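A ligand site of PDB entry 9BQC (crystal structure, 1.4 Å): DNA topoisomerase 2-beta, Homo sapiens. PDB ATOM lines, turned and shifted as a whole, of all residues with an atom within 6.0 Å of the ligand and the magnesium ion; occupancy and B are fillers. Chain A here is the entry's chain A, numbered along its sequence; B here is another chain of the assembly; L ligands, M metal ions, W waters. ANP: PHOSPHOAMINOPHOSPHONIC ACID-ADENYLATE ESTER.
Within 4 Å of the magnesium ion: Asn 66.
The side-chain carboxylate (OE1) of Glu 62 sits close to an oxygen (O1G) of the ligand, at 3.5 Å.
Asn 70 touches the ligand.
Arg 73 touches the ligand (NH1 to C2, 3.8 Å).
CG1 of Ile 100 touches N3 of the ligand, 3.5 Å away.
Ile 116 touches the ligand (CD1 to O4', 3.2 Å).
CZ of Phe 117 touches C8 of the ligand (3.6 Å).
Thr 122 touches the ligand (O to C5', 3.7 Å).
Gly 136 touches the ligand (CA to N3B, 3.5 Å).
Thr 190 touches the ligand.
Tyr 9 of chain B touches the ligand.
Within 4 Å of the ligand: Glu 62, Asn 66, Asn 70, Arg 73, Asn 95, Ile 100, Ile 116, Phe 117, Thr 122, Ser 123, Ser 124, Asn 125, Gly 136, Arg 137, Asn 138, Gly 139, Tyr 140, Gly 141, Ala 142, Lys 143, Thr 190, Gln 351, Lys 353 and Tyr 9 of chain B.
Water W5 lies within hydrogen-bond range of the side-chain carboxylate of Glu 62 (2.6 Å) and the side-chain amide nitrogen of Asn 66 (3.4 Å).
Water W7 lies within hydrogen-bond range of the side-chain hydroxyl (OG1) of Thr 190, a nitrogen (N1) of the ligand, the backbone carbonyl oxygen (O) of Lys 98, the side-chain amide nitrogen (ND2) of Asn 95 and the side-chain amide nitrogen (ND2) of Asn 70.
Water W2 bridges N7 of the ligand and ND2 of Asn 66.
Water W6 lies within hydrogen-bond range of the side-chain hydroxyl of Tyr 9 of chain B (2.7 Å), a nitrogen (N3) of the ligand (2.9 Å) and the guanidinium group of Arg 73 (3.3 Å).
Water W3 lies within hydrogen-bond range of O of Ile 63 (2.9 Å), N6 of the ligand (3.1 Å) and N of Ala 67 (3.5 Å).
Water W4 lies within hydrogen-bond range of OD1 of Asn 70 (3.2 Å) and N3 of the ligand (3.4 Å).
The magnesium ion is bound by an oxygen (O1G) of the ligand, water W5, an oxygen (O1B) of the ligand, the side-chain amide oxygen (OD1) of Asn 66, an oxygen (O2A) of the ligand and water W8.
The magnesium ion has six donor atoms within binding distance.
The side-chain amino group (NZ) of Lys 353 lies within hydrogen-bond range of the backbone carbonyl oxygen (O) of Gly 135, 2.8 Å away.
OG of Ser 123 sits at hydrogen-bond distance from N of Asn 125, 2.8 Å away.
The side-chain hydroxyl (OG1) of Thr 122 sits at hydrogen-bond distance from the side-chain amino group (NZ) of Lys 143 (2.9 Å).
The backbone carbonyl oxygen (O) of Gly 136 sits close to the side-chain amide nitrogen (ND2) of Asn 125, 3.5 Å away.
ND2 of Asn 95 lies close to ND2 of Asn 70 (3.4 Å).
NH1 of Arg 73 sits at hydrogen-bond distance from OD1 of Asn 70 (2.9 Å).
The backbone carbonyl oxygen (O) of Lys 98 lies within hydrogen-bond range of the side-chain amide nitrogen (ND2) of Asn 70 (3.1 Å).
The backbone carbonyl oxygen (O) of Gly 99 lies within hydrogen-bond range of the guanidinium group (NH2) of Arg 73 (3.0 Å).
An oxygen (O3G) of the ligand is in salt-bridge range of the side-chain amino group (NZ) of Lys 353 (2.6 Å).
The side-chain hydroxyl (OG) of Ser 123 lies within hydrogen-bond range of an oxygen (O2B) of the ligand, at 2.6 Å.
N of Ser 124 lies within hydrogen-bond range of O3' of the ligand (3.0 Å).
OG of Ser 124 lies within hydrogen-bond range of O2' of the ligand, 2.7 Å away.
N of Tyr 140 is in hydrogen-bond range of O2G of the ligand (2.8 Å).
The side-chain amino group (NZ) of Lys 143 lies within salt-bridge range of an oxygen (O1A) of the ligand (2.8 Å).
An oxygen (O2G) of the ligand is in hydrogen-bond range of the backbone NH (N) of Gly 141 (2.8 Å).
The backbone NH of Arg 137 lies within hydrogen-bond range of an oxygen (O3G) of the ligand (2.9 Å).
O2B of the ligand sits at hydrogen-bond distance from ND2 of Asn 125, at 2.9 Å.
OD1 of Asn 95 lies within hydrogen-bond range of N6 of the ligand (2.9 Å).
The backbone NH of Ala 142 lies within hydrogen-bond range of an oxygen (O1A) of the ligand.
N of Asn 138 lies within hydrogen-bond range of O3G of the ligand (3.0 Å).
N of Gly 139 is in hydrogen-bond range of O2G of the ligand (3.2 Å).
NE2 of Gln 351 sits at hydrogen-bond distance from O2G of the ligand (3.1 Å).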
ATOM      1  N   GLU A  62     -16.489  14.925  11.647  1.00  0.00           N
ATOM      2  CA  GLU A  62     -16.655  13.541  12.083  1.00  0.00           C
ATOM      3  C   GLU A  62     -16.373  13.400  13.572  1.00  0.00           C
ATOM      4  O   GLU A  62     -17.099  12.696  14.290  1.00  0.00           O
ATOM      5  CB  GLU A  62     -15.731  12.624  11.292  1.00  0.00           C
ATOM      6  CG  GLU A  62     -16.041  12.479   9.799  1.00  0.00           C
ATOM      7  CD  GLU A  62     -17.362  11.749   9.456  1.00  0.00           C
ATOM      8  OE1 GLU A  62     -18.075  11.252  10.362  1.00  0.00           O
ATOM      9  OE2 GLU A  62     -17.706  11.669   8.258  1.00  0.00           O
ATOM     10  N   ILE A  63     -15.335  14.078  14.073  1.00  0.00           N
ATOM     11  CA  ILE A  63     -14.995  13.968  15.479  1.00  0.00           C
ATOM     12  C   ILE A  63     -16.024  14.712  16.329  1.00  0.00           C
ATOM     13  O   ILE A  63     -16.401  14.251  17.404  1.00  0.00           O
ATOM     14  CB  ILE A  63     -13.562  14.468  15.736  1.00  0.00           C
ATOM     15  CG1 ILE A  63     -12.558  13.718  14.834  1.00  0.00           C
ATOM     16  CG2 ILE A  63     -13.205  14.341  17.198  1.00  0.00           C
ATOM     17  CD1 ILE A  63     -12.609  12.168  14.916  1.00  0.00           C
ATOM     18  N   VAL A  65     -19.304  15.246  15.667  1.00  0.00           N
ATOM     19  CA  VAL A  65     -20.542  14.484  15.736  1.00  0.00           C
ATOM     20  C   VAL A  65     -20.364  13.241  16.602  1.00  0.00           C
ATOM     21  O   VAL A  65     -21.272  12.836  17.328  1.00  0.00           O
ATOM     22  CB  VAL A  65     -21.069  14.188  14.325  1.00  0.00           C
ATOM     23  CG1 VAL A  65     -22.284  13.273  14.371  1.00  0.00           C
ATOM     24  CG2 VAL A  65     -21.433  15.496  13.583  1.00  0.00           C
ATOM     25  N   ASN A  66     -19.165  12.634  16.576  1.00  0.00           N
ATOM     26  CA  ASN A  66     -18.921  11.488  17.448  1.00  0.00           C
ATOM     27  C   ASN A  66     -19.069  11.882  18.926  1.00  0.00           C
ATOM     28  O   ASN A  66     -19.554  11.099  19.751  1.00  0.00           O
ATOM     29  CB  ASN A  66     -17.522  10.940  17.221  1.00  0.00           C
ATOM     30  CG  ASN A  66     -17.414  10.038  16.019  1.00  0.00           C
ATOM     31  OD1 ASN A  66     -18.406   9.627  15.434  1.00  0.00           O
ATOM     32  ND2 ASN A  66     -16.177   9.747  15.651  1.00  0.00           N
ATOM     33  N   ALA A  67     -18.622  13.096  19.273  1.00  0.00           N
ATOM     34  CA  ALA A  67     -18.802  13.557  20.654  1.00  0.00           C
ATOM     35  C   ALA A  67     -20.282  13.734  20.978  1.00  0.00           C
ATOM     36  O   ALA A  67     -20.753  13.317  22.044  1.00  0.00           O
ATOM     37  CB  ALA A  67     -18.041  14.866  20.850  1.00  0.00           C
ATOM     38  N   ASP A  69     -22.703  12.164  19.643  1.00  0.00           N
ATOM     39  CA  ASP A  69     -23.276  10.834  19.711  1.00  0.00           C
ATOM     40  C   ASP A  69     -23.124  10.214  21.099  1.00  0.00           C
ATOM     41  O   ASP A  69     -23.912   9.332  21.474  1.00  0.00           O
ATOM     42  CB  ASP A  69     -22.597   9.934  18.666  1.00  0.00           C
ATOM     43  CG  ASP A  69     -23.080  10.170  17.251  1.00  0.00           C
ATOM     44  OD1 ASP A  69     -24.084  10.891  17.055  1.00  0.00           O
ATOM     45  OD2 ASP A  69     -22.432   9.616  16.324  1.00  0.00           O
ATOM     46  N   ASN A  70     -22.111  10.618  21.861  1.00  0.00           N
ATOM     47  CA  ASN A  70     -21.925  10.010  23.170  1.00  0.00           C
ATOM     48  C   ASN A  70     -23.089  10.337  24.094  1.00  0.00           C
ATOM     49  O   ASN A  70     -23.285   9.636  25.083  1.00  0.00           O
ATOM     50  CB  ASN A  70     -20.621  10.450  23.858  1.00  0.00           C
ATOM     51  CG  ASN A  70     -20.162   9.434  24.877  1.00  0.00           C
ATOM     52  OD1 ASN A  70     -20.031   8.250  24.565  1.00  0.00           O
ATOM     53  ND2 ASN A  70     -19.968   9.878  26.122  1.00  0.00           N
ATOM     54  N   ARG A  73     -25.158   7.236  24.209  1.00  0.00           N
ATOM     55  CA  ARG A  73     -24.602   6.167  25.029  1.00  0.00           C
ATOM     56  C   ARG A  73     -24.731   6.485  26.510  1.00  0.00           C
ATOM     57  O   ARG A  73     -24.819   5.566  27.336  1.00  0.00           O
ATOM     58  CB  ARG A  73     -23.104   6.008  24.789  1.00  0.00           C
ATOM     59  CG  ARG A  73     -22.659   5.270  23.553  1.00  0.00           C
ATOM     60  CD  ARG A  73     -21.120   5.136  23.558  1.00  0.00           C
ATOM     61  NE  ARG A  73     -20.616   4.191  24.542  1.00  0.00           N
ATOM     62  CZ  ARG A  73     -19.682   4.467  25.457  1.00  0.00           C
ATOM     63  NH1 ARG A  73     -19.163   5.673  25.579  1.00  0.00           N
ATOM     64  NH2 ARG A  73     -19.247   3.491  26.255  1.00  0.00           N
ATOM     65  N   ASN A  95     -15.115  15.360  25.500  1.00  0.00           N
ATOM     66  CA  ASN A  95     -16.483  15.180  25.962  1.00  0.00           C
ATOM     67  C   ASN A  95     -16.456  14.418  27.277  1.00  0.00           C
ATOM     68  O   ASN A  95     -15.525  13.652  27.543  1.00  0.00           O
ATOM     69  CB  ASN A  95     -17.399  14.459  24.935  1.00  0.00           C
ATOM     70  CG  ASN A  95     -16.998  13.000  24.696  1.00  0.00           C
ATOM     71  OD1 ASN A  95     -16.259  12.691  23.751  1.00  0.00           O
ATOM     72  ND2 ASN A  95     -17.513  12.105  25.530  1.00  0.00           N
ATOM     73  N   LYS A  98     -19.744   8.683  29.644  1.00  0.00           N
ATOM     74  CA  LYS A  98     -19.008   7.428  29.691  1.00  0.00           C
ATOM     75  C   LYS A  98     -17.879   7.410  28.667  1.00  0.00           C
ATOM     76  O   LYS A  98     -18.056   7.804  27.515  1.00  0.00           O
ATOM     77  CB  LYS A  98     -19.976   6.288  29.391  1.00  0.00           C
ATOM     78  CG  LYS A  98     -19.485   4.903  29.803  1.00  0.00           C
ATOM     79  CD  LYS A  98     -20.626   3.901  29.823  1.00  0.00           C
ATOM     80  CE  LYS A  98     -20.128   2.500  30.189  1.00  0.00           C
ATOM     81  NZ  LYS A  98     -19.374   2.488  31.473  1.00  0.00           N
ATOM     82  N   GLY A  99     -16.719   6.930  29.111  1.00  0.00           N
ATOM     83  CA  GLY A  99     -15.612   6.702  28.212  1.00  0.00           C
ATOM     84  C   GLY A  99     -15.805   5.427  27.403  1.00  0.00           C
ATOM     85  O   GLY A  99     -16.848   4.770  27.449  1.00  0.00           O
ATOM     86  N   ILE A 100     -14.751   5.069  26.666  1.00  0.00           N
ATOM     87  CA  ILE A 100     -14.777   3.853  25.850  1.00  0.00           C
ATOM     88  C   ILE A 100     -14.145   2.729  26.658  1.00  0.00           C
ATOM     89  O   ILE A 100     -13.087   2.935  27.271  1.00  0.00           O
ATOM     90  CB  ILE A 100     -14.034   4.089  24.532  1.00  0.00           C
ATOM     91  CG1 ILE A 100     -14.737   5.196  23.758  1.00  0.00           C
ATOM     92  CG2 ILE A 100     -13.981   2.801  23.729  1.00  0.00           C
ATOM     93  CD1 ILE A 100     -13.866   5.852  22.727  1.00  0.00           C
ATOM     94  N   ILE A 116     -11.489   0.729  17.123  1.00  0.00           N
ATOM     95  CA  ILE A 116     -12.509   1.597  16.553  1.00  0.00           C
ATOM     96  C   ILE A 116     -11.979   2.939  16.080  1.00  0.00           C
ATOM     97  O   ILE A 116     -12.692   3.662  15.390  1.00  0.00           O
ATOM     98  CB  ILE A 116     -13.725   1.708  17.492  1.00  0.00           C
ATOM     99  CG1 ILE A 116     -13.379   2.538  18.736  1.00  0.00           C
ATOM    100  CG2 ILE A 116     -14.235   0.311  17.870  1.00  0.00           C
ATOM    101  CD1 ILE A 116     -14.499   2.576  19.742  1.00  0.00           C
ATOM    102  N   PHE A 117     -10.727   3.287  16.415  1.00  0.00           N
ATOM    103  CA  PHE A 117     -10.071   4.464  15.856  1.00  0.00           C
ATOM    104  C   PHE A 117      -8.963   4.121  14.866  1.00  0.00           C
ATOM    105  O   PHE A 117      -8.506   5.025  14.157  1.00  0.00           O
ATOM    106  CB  PHE A 117      -9.502   5.348  16.981  1.00  0.00           C
ATOM    107  CG  PHE A 117     -10.545   6.083  17.738  1.00  0.00           C
ATOM    108  CD1 PHE A 117     -11.014   7.297  17.270  1.00  0.00           C
ATOM    109  CD2 PHE A 117     -11.085   5.549  18.897  1.00  0.00           C
ATOM    110  CE1 PHE A 117     -11.997   7.975  17.950  1.00  0.00           C
ATOM    111  CE2 PHE A 117     -12.069   6.230  19.590  1.00  0.00           C
ATOM    112  CZ  PHE A 117     -12.529   7.447  19.108  1.00  0.00           C
ATOM    113  N   THR A 122     -15.447  -0.176  11.574  1.00  0.00           N
ATOM    114  CA  THR A 122     -15.627  -0.543  12.977  1.00  0.00           C
ATOM    115  C   THR A 122     -16.577   0.457  13.617  1.00  0.00           C
ATOM    116  O   THR A 122     -16.426   1.672  13.427  1.00  0.00           O
ATOM    117  CB  THR A 122     -14.284  -0.559  13.717  1.00  0.00           C
ATOM    118  OG1 THR A 122     -13.589   0.676  13.526  1.00  0.00           O
ATOM    119  CG2 THR A 122     -13.398  -1.709  13.236  1.00  0.00           C
ATOM    120  N   SER A 123     -17.557  -0.048  14.374  1.00  0.00           N
ATOM    121  CA  SER A 123     -18.646   0.816  14.831  1.00  0.00           C
ATOM    122  C   SER A 123     -19.435   0.142  15.937  1.00  0.00           C
ATOM    123  O   SER A 123     -19.491  -1.081  15.998  1.00  0.00           O
ATOM    124  CB  SER A 123     -19.601   1.116  13.664  1.00  0.00           C
ATOM    125  OG  SER A 123     -20.631   2.041  14.017  1.00  0.00           O
ATOM    126  N   SER A 124     -20.061   0.962  16.778  1.00  0.00           N
ATOM    127  CA  SER A 124     -21.113   0.520  17.669  1.00  0.00           C
ATOM    128  C   SER A 124     -22.493   0.757  17.073  1.00  0.00           C
ATOM    129  O   SER A 124     -23.502   0.535  17.752  1.00  0.00           O
ATOM    130  CB  SER A 124     -21.000   1.223  19.025  1.00  0.00           C
ATOM    131  OG  SER A 124     -21.123   2.629  18.867  1.00  0.00           O
ATOM    132  N   ASN A 125     -22.561   1.173  15.801  1.00  0.00           N
ATOM    133  CA  ASN A 125     -23.819   1.542  15.156  1.00  0.00           C
ATOM    134  C   ASN A 125     -24.230   0.594  14.027  1.00  0.00           C
ATOM    135  O   ASN A 125     -25.037   0.984  13.171  1.00  0.00           O
ATOM    136  CB  ASN A 125     -23.730   2.971  14.631  1.00  0.00           C
ATOM    137  CG  ASN A 125     -23.672   3.976  15.750  1.00  0.00           C
ATOM    138  OD1 ASN A 125     -24.611   4.079  16.530  1.00  0.00           O
ATOM    139  ND2 ASN A 125     -22.560   4.677  15.874  1.00  0.00           N
ATOM    140  N   GLY A 135     -25.707  10.138  15.048  1.00  0.00           N
ATOM    141  CA  GLY A 135     -25.329  10.477  13.688  1.00  0.00           C
ATOM    142  C   GLY A 135     -24.467   9.425  13.038  1.00  0.00           C
ATOM    143  O   GLY A 135     -24.511   9.254  11.809  1.00  0.00           O
ATOM    144  N   GLY A 136     -23.690   8.696  13.828  1.00  0.00           N
ATOM    145  CA  GLY A 136     -22.832   7.644  13.287  1.00  0.00           C
ATOM    146  C   GLY A 136     -23.632   6.467  12.754  1.00  0.00           C
ATOM    147  O   GLY A 136     -24.579   5.986  13.378  1.00  0.00           O
ATOM    148  N   ARG A 137     -23.211   5.988  11.569  1.00  0.00           N
ATOM    149  CA  ARG A 137     -23.864   4.866  10.903  1.00  0.00           C
ATOM    150  C   ARG A 137     -22.894   3.901  10.235  1.00  0.00           C
ATOM    151  O   ARG A 137     -23.214   2.714  10.131  1.00  0.00           O
ATOM    152  CB  ARG A 137     -24.832   5.380   9.820  1.00  0.00           C
ATOM    153  CG  ARG A 137     -25.847   6.419  10.316  1.00  0.00           C
ATOM    154  CD  ARG A 137     -26.884   5.807  11.238  1.00  0.00           C
ATOM    155  NE  ARG A 137     -27.723   4.848  10.516  1.00  0.00           N
ATOM    156  CZ  ARG A 137     -27.971   3.601  10.887  1.00  0.00           C
ATOM    157  NH1 ARG A 137     -27.606   3.143  12.081  1.00  0.00           N
ATOM    158  NH2 ARG A 137     -28.602   2.785  10.047  1.00  0.00           N
ATOM    159  N   ASN A 138     -21.723   4.354   9.786  1.00  0.00           N
ATOM    160  CA  ASN A 138     -20.959   3.598   8.796  1.00  0.00           C
ATOM    161  C   ASN A 138     -19.650   3.004   9.276  1.00  0.00           C
ATOM    162  O   ASN A 138     -19.115   2.107   8.605  1.00  0.00           O
ATOM    163  CB  ASN A 138     -20.663   4.474   7.573  1.00  0.00           C
ATOM    164  CG  ASN A 138     -21.919   5.011   6.935  1.00  0.00           C
ATOM    165  OD1 ASN A 138     -22.933   4.320   6.882  1.00  0.00           O
ATOM    166  ND2 ASN A 138     -21.859   6.247   6.451  1.00  0.00           N
ATOM    167  N   GLY A 139     -19.104   3.461  10.399  1.00  0.00           N
ATOM    168  CA  GLY A 139     -17.846   2.919  10.879  1.00  0.00           C
ATOM    169  C   GLY A 139     -16.608   3.419  10.185  1.00  0.00           C
ATOM    170  O   GLY A 139     -15.576   2.738  10.185  1.00  0.00           O
ATOM    171  N   TYR A 140     -16.662   4.633   9.632  1.00  0.00           N
ATOM    172  CA  TYR A 140     -15.536   5.271   8.957  1.00  0.00           C
ATOM    173  C   TYR A 140     -15.026   6.538   9.624  1.00  0.00           C
ATOM    174  O   TYR A 140     -13.812   6.809   9.581  1.00  0.00           O
ATOM    175  CB  TYR A 140     -15.951   5.704   7.547  1.00  0.00           C
ATOM    176  CG  TYR A 140     -15.765   4.707   6.444  1.00  0.00           C
ATOM    177  CD1 TYR A 140     -14.505   4.268   6.103  1.00  0.00           C
ATOM    178  CD2 TYR A 140     -16.839   4.269   5.692  1.00  0.00           C
ATOM    179  CE1 TYR A 140     -14.322   3.370   5.072  1.00  0.00           C
ATOM    180  CE2 TYR A 140     -16.669   3.369   4.654  1.00  0.00           C
ATOM    181  CZ  TYR A 140     -15.407   2.932   4.349  1.00  0.00           C
ATOM    182  OH  TYR A 140     -15.184   2.046   3.318  1.00  0.00           O
ATOM    183  N   GLY A 141     -15.919   7.382  10.164  1.00  0.00           N
ATOM    184  CA  GLY A 141     -15.587   8.791  10.417  1.00  0.00           C
ATOM    185  C   GLY A 141     -14.294   9.065  11.162  1.00  0.00           C
ATOM    186  O   GLY A 141     -13.470   9.872  10.712  1.00  0.00           O
ATOM    187  N   ALA A 142     -14.094   8.382  12.285  1.00  0.00           N
ATOM    188  CA  ALA A 142     -12.885   8.640  13.072  1.00  0.00           C
ATOM    189  C   ALA A 142     -11.631   8.164  12.347  1.00  0.00           C
ATOM    190  O   ALA A 142     -10.574   8.774  12.486  1.00  0.00           O
ATOM    191  CB  ALA A 142     -12.993   7.984  14.449  1.00  0.00           C
ATOM    192  N   LYS A 143     -11.707   7.028  11.625  1.00  0.00           N
ATOM    193  CA  LYS A 143     -10.553   6.580  10.850  1.00  0.00           C
ATOM    194  C   LYS A 143     -10.227   7.564   9.736  1.00  0.00           C
ATOM    195  O   LYS A 143      -9.054   7.773   9.420  1.00  0.00           O
ATOM    196  CB  LYS A 143     -10.803   5.189  10.273  1.00  0.00           C
ATOM    197  CG  LYS A 143     -10.557   4.016  11.238  1.00  0.00           C
ATOM    198  CD  LYS A 143     -11.595   3.941  12.368  1.00  0.00           C
ATOM    199  CE  LYS A 143     -12.992   3.600  11.862  1.00  0.00           C
ATOM    200  NZ  LYS A 143     -14.018   3.451  12.951  1.00  0.00           N
ATOM    201  N   THR A 190     -13.583  11.394  27.026  1.00  0.00           N
ATOM    202  CA  THR A 190     -12.817  11.053  25.829  1.00  0.00           C
ATOM    203  C   THR A 190     -12.330  12.353  25.224  1.00  0.00           C
ATOM    204  O   THR A 190     -13.058  13.342  25.179  1.00  0.00           O
ATOM    205  CB  THR A 190     -13.685  10.304  24.827  1.00  0.00           C
ATOM    206  OG1 THR A 190     -14.064   9.038  25.389  1.00  0.00           O
ATOM    207  CG2 THR A 190     -12.948  10.074  23.516  1.00  0.00           C
ATOM    208  N   ILE A 192     -10.138  13.629  21.759  1.00  0.00           N
ATOM    209  CA  ILE A 192      -9.480  13.359  20.487  1.00  0.00           C
ATOM    210  C   ILE A 192      -8.696  14.620  20.116  1.00  0.00           C
ATOM    211  O   ILE A 192      -9.276  15.707  20.016  1.00  0.00           O
ATOM    212  CB  ILE A 192     -10.510  13.025  19.397  1.00  0.00           C
ATOM    213  CG1 ILE A 192     -11.447  11.898  19.851  1.00  0.00           C
ATOM    214  CG2 ILE A 192      -9.811  12.709  18.073  1.00  0.00           C
ATOM    215  CD1 ILE A 192     -10.750  10.671  20.403  1.00  0.00           C
ATOM    216  N   GLN A 351     -20.999   9.442   2.670  1.00  0.00           N
ATOM    217  CA  GLN A 351     -20.397   9.508   3.999  1.00  0.00           C
ATOM    218  C   GLN A 351     -20.446  10.931   4.554  1.00  0.00           C
ATOM    219  O   GLN A 351     -20.471  11.096   5.786  1.00  0.00           O
ATOM    220  CB  GLN A 351     -18.947   8.999   3.970  1.00  0.00           C
ATOM    221  CG  GLN A 351     -18.184   9.167   5.288  1.00  0.00           C
ATOM    222  CD  GLN A 351     -18.649   8.232   6.367  1.00  0.00           C
ATOM    223  OE1 GLN A 351     -19.140   7.139   6.084  1.00  0.00           O
ATOM    224  NE2 GLN A 351     -18.507   8.647   7.621  1.00  0.00           N
ATOM    225  N   LYS A 353     -22.852  12.960   4.521  1.00  0.00           N
ATOM    226  CA  LYS A 353     -24.149  13.114   5.183  1.00  0.00           C
ATOM    227  C   LYS A 353     -24.768  14.496   4.979  1.00  0.00           C
ATOM    228  O   LYS A 353     -25.437  15.024   5.867  1.00  0.00           O
ATOM    229  CB  LYS A 353     -24.040  12.768   6.660  1.00  0.00           C
ATOM    230  CG  LYS A 353     -23.578  11.351   6.903  1.00  0.00           C
ATOM    231  CD  LYS A 353     -23.425  11.027   8.372  1.00  0.00           C
ATOM    232  CE  LYS A 353     -22.733   9.698   8.569  1.00  0.00           C
ATOM    233  NZ  LYS A 353     -22.335   9.511   9.996  1.00  0.00           N
ATOM    234  N   TYR B   9     -19.259  -3.465  19.891  1.00  0.00           N
ATOM    235  CA  TYR B   9     -18.259  -2.956  18.960  1.00  0.00           C
ATOM    236  C   TYR B   9     -17.968  -4.037  17.926  1.00  0.00           C
ATOM    237  O   TYR B   9     -17.434  -5.099  18.271  1.00  0.00           O
ATOM    238  CB  TYR B   9     -17.003  -2.547  19.702  1.00  0.00           C
ATOM    239  CG  TYR B   9     -17.276  -1.458  20.721  1.00  0.00           C
ATOM    240  CD1 TYR B   9     -17.376  -0.130  20.313  1.00  0.00           C
ATOM    241  CD2 TYR B   9     -17.470  -1.748  22.048  1.00  0.00           C
ATOM    242  CE1 TYR B   9     -17.614   0.879  21.207  1.00  0.00           C
ATOM    243  CE2 TYR B   9     -17.710  -0.733  22.968  1.00  0.00           C
ATOM    244  CZ  TYR B   9     -17.799   0.575  22.523  1.00  0.00           C
ATOM    245  OH  TYR B   9     -18.039   1.573  23.447  1.00  0.00           O
HETATM  246  PG  ANP L   1     -19.689   7.056  10.925  1.00  0.00           P
HETATM  247  O1G ANP L   1     -19.237   8.279  11.691  1.00  0.00           O
HETATM  248  O2G ANP L   1     -18.608   6.563   9.922  1.00  0.00           O
HETATM  249  O3G ANP L   1     -21.039   7.231  10.156  1.00  0.00           O
HETATM  250  PB  ANP L   1     -19.410   5.767  13.558  1.00  0.00           P
HETATM  251  O1B ANP L   1     -19.526   7.053  14.327  1.00  0.00           O
HETATM  252  O2B ANP L   1     -20.072   4.605  14.316  1.00  0.00           O
HETATM  253  N3B ANP L   1     -20.098   5.830  12.042  1.00  0.00           N
HETATM  254  PA  ANP L   1     -16.593   6.305  13.777  1.00  0.00           P
HETATM  255  O1A ANP L   1     -15.422   5.821  13.025  1.00  0.00           O
HETATM  256  O2A ANP L   1     -16.919   7.786  13.624  1.00  0.00           O
HETATM  257  O3A ANP L   1     -17.871   5.470  13.329  1.00  0.00           O
HETATM  258  O5' ANP L   1     -16.438   5.952  15.303  1.00  0.00           O
HETATM  259  C5' ANP L   1     -16.145   4.593  15.659  1.00  0.00           C
HETATM  260  C4' ANP L   1     -16.766   4.240  16.975  1.00  0.00           C
HETATM  261  O4' ANP L   1     -15.994   4.855  18.015  1.00  0.00           O
HETATM  262  C3' ANP L   1     -18.190   4.734  17.176  1.00  0.00           C
HETATM  263  O3' ANP L   1     -19.130   3.816  16.648  1.00  0.00           O
HETATM  264  C2' ANP L   1     -18.274   4.843  18.692  1.00  0.00           C
HETATM  265  O2' ANP L   1     -18.584   3.569  19.268  1.00  0.00           O
HETATM  266  C1' ANP L   1     -16.843   5.177  19.108  1.00  0.00           C
HETATM  267  N9  ANP L   1     -16.606   6.576  19.457  1.00  0.00           N
HETATM  268  C8  ANP L   1     -16.100   7.555  18.656  1.00  0.00           C
HETATM  269  N7  ANP L   1     -15.970   8.720  19.237  1.00  0.00           N
HETATM  270  C5  ANP L   1     -16.409   8.473  20.536  1.00  0.00           C
HETATM  271  C6  ANP L   1     -16.527   9.311  21.665  1.00  0.00           C
HETATM  272  N6  ANP L   1     -16.207  10.606  21.665  1.00  0.00           N
HETATM  273  N1  ANP L   1     -16.991   8.757  22.805  1.00  0.00           N
HETATM  274  C2  ANP L   1     -17.335   7.462  22.802  1.00  0.00           C
HETATM  275  N3  ANP L   1     -17.265   6.584  21.795  1.00  0.00           N
HETATM  276  C4  ANP L   1     -16.787   7.157  20.681  1.00  0.00           C
HETATM  277 MG    MG M   1     -18.755   8.808  13.541  1.00  0.00          MG
HETATM  278  O   HOH W   1     -19.450   8.306  19.305  1.00  0.00           O
HETATM  279  O   HOH W   2     -14.326  10.585  17.838  1.00  0.00           O
HETATM  280  O   HOH W   3     -15.202  12.611  19.528  1.00  0.00           O
HETATM  281  O   HOH W   4     -20.567   7.220  21.595  1.00  0.00           O
HETATM  282  O   HOH W   5     -17.843  10.499  12.831  1.00  0.00           O
HETATM  283  O   HOH W   6     -18.341   3.961  22.205  1.00  0.00           O
HETATM  284  O   HOH W   7     -16.653   9.286  25.551  1.00  0.00           O
HETATM  285  O   HOH W   8     -20.587   9.928  13.742  1.00  0.00           O
HETATM  286  O   HOH W   9     -20.650   7.689  16.892  1.00  0.00           O
